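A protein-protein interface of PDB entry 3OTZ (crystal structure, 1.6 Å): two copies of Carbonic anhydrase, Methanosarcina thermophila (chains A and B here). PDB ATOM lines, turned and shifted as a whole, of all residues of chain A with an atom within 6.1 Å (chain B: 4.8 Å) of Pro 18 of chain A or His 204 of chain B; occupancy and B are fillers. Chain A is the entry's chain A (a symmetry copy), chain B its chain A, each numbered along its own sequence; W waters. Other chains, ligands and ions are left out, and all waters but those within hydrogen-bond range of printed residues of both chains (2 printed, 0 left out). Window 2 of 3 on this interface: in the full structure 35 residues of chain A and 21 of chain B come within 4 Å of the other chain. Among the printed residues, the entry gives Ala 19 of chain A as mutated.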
ATOM      1  N   VAL A  16      22.061 -14.856  14.669  1.00  0.00           N
ATOM      2  CA  VAL A  16      23.052 -15.148  15.704  1.00  0.00           C
ATOM      3  C   VAL A  16      23.525 -13.835  16.326  1.00  0.00           C
ATOM      4  O   VAL A  16      23.890 -12.898  15.608  1.00  0.00           O
ATOM      5  CB  VAL A  16      24.273 -15.883  15.108  1.00  0.00           C
ATOM      6  CG1 VAL A  16      25.360 -16.086  16.178  1.00  0.00           C
ATOM      7  CG2 VAL A  16      23.838 -17.212  14.505  1.00  0.00           C
ATOM      8  N   THR A  17      23.499 -13.768  17.656  1.00  0.00           N
ATOM      9  CA  THR A  17      23.992 -12.611  18.403  1.00  0.00           C
ATOM     10  C   THR A  17      24.826 -13.130  19.564  1.00  0.00           C
ATOM     11  O   THR A  17      24.846 -14.338  19.812  1.00  0.00           O
ATOM     12  CB  THR A  17      22.832 -11.754  18.984  1.00  0.00           C
ATOM     13  OG1 THR A  17      22.125 -12.516  19.969  1.00  0.00           O
ATOM     14  CG2 THR A  17      21.860 -11.316  17.881  1.00  0.00           C
ATOM     15  N   PRO A  18      25.515 -12.225  20.283  1.00  0.00           N
ATOM     16  CA  PRO A  18      26.328 -12.693  21.419  1.00  0.00           C
ATOM     17  C   PRO A  18      25.515 -13.417  22.501  1.00  0.00           C
ATOM     18  O   PRO A  18      26.084 -14.200  23.263  1.00  0.00           O
ATOM     19  CB  PRO A  18      26.975 -11.406  21.959  1.00  0.00           C
ATOM     20  CG  PRO A  18      26.215 -10.267  21.323  1.00  0.00           C
ATOM     21  CD  PRO A  18      25.694 -10.785  20.018  1.00  0.00           C
ATOM     22  N   ALA A  19      24.206 -13.180  22.545  1.00  0.00           N
ATOM     23  CA  ALA A  19      23.337 -13.840  23.519  1.00  0.00           C
ATOM     24  C   ALA A  19      22.466 -14.930  22.886  1.00  0.00           C
ATOM     25  O   ALA A  19      21.626 -15.526  23.560  1.00  0.00           O
ATOM     26  CB  ALA A  19      22.462 -12.811  24.210  1.00  0.00           C
ATOM     27  N   ASN A  20      22.670 -15.186  21.595  1.00  0.00           N
ATOM     28  CA  ASN A  20      21.890 -16.171  20.850  1.00  0.00           C
ATOM     29  C   ASN A  20      22.787 -16.971  19.905  1.00  0.00           C
ATOM     30  O   ASN A  20      22.870 -16.652  18.719  1.00  0.00           O
ATOM     31  CB  ASN A  20      20.785 -15.469  20.047  1.00  0.00           C
ATOM     32  CG  ASN A  20      19.775 -16.443  19.456  1.00  0.00           C
ATOM     33  OD1 ASN A  20      18.993 -17.057  20.186  1.00  0.00           O
ATOM     34  ND2 ASN A  20      19.772 -16.575  18.132  1.00  0.00           N
ATOM     35  N   PRO A  21      23.459 -18.013  20.431  1.00  0.00           N
ATOM     36  CA  PRO A  21      24.382 -18.871  19.672  1.00  0.00           C
ATOM     37  C   PRO A  21      23.705 -19.725  18.601  1.00  0.00           C
ATOM     38  O   PRO A  21      24.338 -20.030  17.587  1.00  0.00           O
ATOM     39  CB  PRO A  21      24.980 -19.789  20.750  1.00  0.00           C
ATOM     40  CG  PRO A  21      24.707 -19.114  22.048  1.00  0.00           C
ATOM     41  CD  PRO A  21      23.423 -18.376  21.857  1.00  0.00           C
ATOM     42  N   ASN A  87      21.945 -12.320  29.004  1.00  0.00           N
ATOM     43  CA  ASN A  87      22.952 -11.301  28.724  1.00  0.00           C
ATOM     44  C   ASN A  87      24.118 -11.890  27.913  1.00  0.00           C
ATOM     45  O   ASN A  87      24.126 -13.081  27.588  1.00  0.00           O
ATOM     46  CB  ASN A  87      23.434 -10.609  30.013  1.00  0.00           C
ATOM     47  CG  ASN A  87      24.344 -11.482  30.848  1.00  0.00           C
ATOM     48  OD1 ASN A  87      24.837 -12.509  30.387  1.00  0.00           O
ATOM     49  ND2 ASN A  87      24.578 -11.070  32.087  1.00  0.00           N
ATOM     50  N   GLU A  88      25.088 -11.045  27.572  1.00  0.00           N
ATOM     51  CA  GLU A  88      26.214 -11.465  26.739  1.00  0.00           C
ATOM     52  C   GLU A  88      27.048 -12.559  27.397  1.00  0.00           C
ATOM     53  O   GLU A  88      27.730 -13.327  26.720  1.00  0.00           O
ATOM     54  CB  GLU A  88      27.099 -10.266  26.420  1.00  0.00           C
ATOM     55  CG  GLU A  88      26.603  -9.447  25.254  1.00  0.00           C
ATOM     56  CD  GLU A  88      27.646  -8.485  24.775  1.00  0.00           C
ATOM     57  OE1 GLU A  88      27.960  -7.560  25.546  1.00  0.00           O
ATOM     58  OE2 GLU A  88      28.161  -8.662  23.649  1.00  0.00           O
ATOM     59  N   GLU A  89      26.987 -12.616  28.723  1.00  0.00           N
ATOM     60  CA  GLU A  89      27.736 -13.594  29.498  1.00  0.00           C
ATOM     61  C   GLU A  89      26.935 -14.881  29.738  1.00  0.00           C
ATOM     62  O   GLU A  89      27.261 -15.667  30.628  1.00  0.00           O
ATOM     63  CB  GLU A  89      28.147 -12.961  30.827  1.00  0.00           C
ATOM     64  CG  GLU A  89      28.955 -11.677  30.654  1.00  0.00           C
ATOM     65  CD  GLU A  89      29.080 -10.875  31.936  1.00  0.00           C
ATOM     66  OE1 GLU A  89      28.314 -11.140  32.883  1.00  0.00           O
ATOM     67  OE2 GLU A  89      29.947  -9.976  31.996  1.00  0.00           O
ATOM     68  N   GLY A  90      25.894 -15.090  28.933  1.00  0.00           N
ATOM     69  CA  GLY A  90      25.043 -16.266  29.045  1.00  0.00           C
ATOM     70  C   GLY A  90      24.195 -16.309  30.306  1.00  0.00           C
ATOM     71  O   GLY A  90      23.531 -17.307  30.582  1.00  0.00           O
ATOM     72  N   TYR B 200      22.717  -0.847  22.621  1.00  0.00           N
ATOM     73  CA  TYR B 200      23.736  -1.899  22.571  1.00  0.00           C
ATOM     74  C   TYR B 200      23.176  -3.140  21.891  1.00  0.00           C
ATOM     75  O   TYR B 200      23.792  -3.716  20.974  1.00  0.00           O
ATOM     76  CB  TYR B 200      24.179  -2.250  23.988  1.00  0.00           C
ATOM     77  CG  TYR B 200      25.299  -3.238  24.018  1.00  0.00           C
ATOM     78  CD1 TYR B 200      26.619  -2.828  23.838  1.00  0.00           C
ATOM     79  CD2 TYR B 200      25.043  -4.576  24.215  1.00  0.00           C
ATOM     80  CE1 TYR B 200      27.659  -3.733  23.868  1.00  0.00           C
ATOM     81  CE2 TYR B 200      26.097  -5.504  24.247  1.00  0.00           C
ATOM     82  CZ  TYR B 200      27.390  -5.063  24.068  1.00  0.00           C
ATOM     83  OH  TYR B 200      28.451  -5.936  24.089  1.00  0.00           O
ATOM     84  N   VAL B 201      21.994  -3.551  22.329  1.00  0.00           N
ATOM     85  CA  VAL B 201      21.363  -4.732  21.734  1.00  0.00           C
ATOM     86  C   VAL B 201      21.039  -4.538  20.256  1.00  0.00           C
ATOM     87  O   VAL B 201      21.276  -5.440  19.453  1.00  0.00           O
ATOM     88  CB  VAL B 201      20.055  -5.055  22.490  1.00  0.00           C
ATOM     89  CG1 VAL B 201      19.232  -6.085  21.716  1.00  0.00           C
ATOM     90  CG2 VAL B 201      20.389  -5.559  23.878  1.00  0.00           C
ATOM     91  N   ASN B 202      20.498  -3.397  19.870  1.00  0.00           N
ATOM     92  CA  ASN B 202      20.077  -3.190  18.495  1.00  0.00           C
ATOM     93  C   ASN B 202      21.242  -3.047  17.544  1.00  0.00           C
ATOM     94  O   ASN B 202      21.124  -3.433  16.388  1.00  0.00           O
ATOM     95  CB  ASN B 202      19.144  -1.986  18.341  1.00  0.00           C
ATOM     96  CG  ASN B 202      17.687  -2.343  18.645  1.00  0.00           C
ATOM     97  OD1 ASN B 202      16.939  -2.739  17.743  1.00  0.00           O
ATOM     98  ND2 ASN B 202      17.289  -2.209  19.898  1.00  0.00           N
ATOM     99  N   VAL B 203      22.375  -2.497  17.990  1.00  0.00           N
ATOM    100  CA  VAL B 203      23.546  -2.457  17.104  1.00  0.00           C
ATOM    101  C   VAL B 203      23.986  -3.885  16.830  1.00  0.00           C
ATOM    102  O   VAL B 203      24.351  -4.224  15.704  1.00  0.00           O
ATOM    103  CB  VAL B 203      24.664  -1.613  17.746  1.00  0.00           C
ATOM    104  CG1 VAL B 203      26.048  -1.895  17.088  1.00  0.00           C
ATOM    105  CG2 VAL B 203      24.291  -0.113  17.626  1.00  0.00           C
ATOM    106  N   HIS B 204      23.935  -4.757  17.843  1.00  0.00           N
ATOM    107  CA  HIS B 204      24.291  -6.166  17.601  1.00  0.00           C
ATOM    108  C   HIS B 204      23.274  -6.923  16.782  1.00  0.00           C
ATOM    109  O   HIS B 204      23.648  -7.801  15.979  1.00  0.00           O
ATOM    110  CB  HIS B 204      24.530  -6.882  18.922  1.00  0.00           C
ATOM    111  CG  HIS B 204      25.843  -6.510  19.541  1.00  0.00           C
ATOM    112  ND1 HIS B 204      26.007  -5.369  20.292  1.00  0.00           N
ATOM    113  CD2 HIS B 204      27.071  -7.073  19.442  1.00  0.00           C
ATOM    114  CE1 HIS B 204      27.270  -5.269  20.671  1.00  0.00           C
ATOM    115  NE2 HIS B 204      27.934  -6.296  20.177  1.00  0.00           N
ATOM    116  N   LEU B 205      21.994  -6.608  16.970  1.00  0.00           N
ATOM    117  CA  LEU B 205      20.972  -7.223  16.113  1.00  0.00           C
ATOM    118  C   LEU B 205      21.144  -6.824  14.656  1.00  0.00           C
ATOM    119  O   LEU B 205      20.978  -7.667  13.760  1.00  0.00           O
ATOM    120  CB  LEU B 205      19.538  -6.840  16.571  1.00  0.00           C
ATOM    121  CG  LEU B 205      19.010  -7.560  17.801  1.00  0.00           C
ATOM    122  CD1 LEU B 205      17.695  -6.882  18.236  1.00  0.00           C
ATOM    123  CD2 LEU B 205      18.818  -9.036  17.491  1.00  0.00           C
ATOM    124  N   ALA B 206      21.458  -5.554  14.391  1.00  0.00           N
ATOM    125  CA  ALA B 206      21.645  -5.096  13.016  1.00  0.00           C
ATOM    126  C   ALA B 206      22.739  -5.922  12.350  1.00  0.00           C
ATOM    127  O   ALA B 206      22.596  -6.340  11.201  1.00  0.00           O
ATOM    128  CB  ALA B 206      21.985  -3.601  12.988  1.00  0.00           C
ATOM    129  N   GLU B 207      23.837  -6.174  13.066  1.00  0.00           N
ATOM    130  CA  GLU B 207      24.942  -6.935  12.480  1.00  0.00           C
ATOM    131  C   GLU B 207      24.516  -8.385  12.238  1.00  0.00           C
ATOM    132  O   GLU B 207      24.828  -8.982  11.207  1.00  0.00           O
ATOM    133  CB  GLU B 207      26.140  -6.886  13.429  1.00  0.00           C
ATOM    134  CG  GLU B 207      27.346  -7.715  12.937  1.00  0.00           C
ATOM    135  CD  GLU B 207      27.824  -7.372  11.514  1.00  0.00           C
ATOM    136  OE1 GLU B 207      27.344  -6.385  10.906  1.00  0.00           O
ATOM    137  OE2 GLU B 207      28.701  -8.105  11.004  1.00  0.00           O
ATOM    138  N   GLY B 208      23.777  -8.969  13.181  1.00  0.00           N
ATOM    139  CA  GLY B 208      23.309 -10.334  12.995  1.00  0.00           C
ATOM    140  C   GLY B 208      22.327 -10.461  11.824  1.00  0.00           C
ATOM    141  O   GLY B 208      22.415 -11.437  11.043  1.00  0.00           O
HETATM  142  O   HOH W   1      25.373 -10.082  16.207  1.00  0.00           O
HETATM  143  O   HOH W   2      22.992 -14.188  11.934  1.00  0.00           O
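Water W1 bridges the backbone carbonyl oxygen of His 204 of chain B (2.9 Å) and the backbone carbonyl oxygen of Val 16 of chain A (3.2 Å). Water W2 lies within hydrogen-bond range of O of Gly 208 of chain B (2.9 Å) and N of Val 16 of chain A (3.0 Å).
The side-chain carboxylate (OE2) of Glu 88 of chain A lies close to the side-chain hydroxyl (OH) of Tyr 200 of chain B (2.8 Å).
No position is printed for both chains. Of the 4 pairs that touch across the chains among the printed residues, none has its exchanged pair printed and touching as well.
Among the printed residues, merely in contact across the chains: Val 16 of chain A with Gly 208 of chain B (3.7 Å), Thr 17 of chain A with Leu 205 of chain B (3.8 Å) and Pro 18 of chain A with His 204 of chain B (3.8 Å).
Printed residues of chain B within 4 Å of Val 16 of chain A: Gly 208. Of the printed residues of chain B, Thr 17 of chain A touches Leu 205. Pro 18 of chain A touches just one residue of chain B: His 204. Printed residues of chain B within 4 Å of Glu 88 of chain A: Tyr 200. Asn 202 of chain B touches none of the printed residues of chain A. Val 203 of chain B touches none of the printed residues of chain A. Of chain A, only Pro 18 comes within 4 Å of His 204 of chain B. Printed residues of chain A within 4 Å of Leu 205 of chain B: Thr 17. Printed residues of chain A within 4 Å of Gly 208 of chain B: Val 16 (3.7 Å). The nearest printed residue of chain B that does not touch Val 16 of chain A is His 204 of chain B (5.1 Å).
Of the 10 printed residues of chain A, 4 touch a printed residue of chain B. Printed residues of chain A that touch a printed residue of chain B: Val 16, Thr 17, Pro 18 and Glu 88. Of the 9 printed residues of chain B, 4 touch a printed residue of chain A. Printed residues of chain B that touch a printed residue of chain A: Tyr 200, His 204, Leu 205 and Gly 208. Along chain B the printed residues that touch a printed residue of chain A span positions 200 to 208. Among the printed residues, 4 pairs touch across the chains.
The backbone carbonyl oxygen (O) of Tyr 200 of chain B sits at hydrogen-bond distance from a ring nitrogen (ND1) of His 204 of chain B. The side-chain hydroxyl of Thr 17 of chain A lies within hydrogen-bond range of the backbone NH of Asn 20 of chain A. OG1 of Thr 17 of chain A sits close to N of Ala 19 of chain A (3.4 Å).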
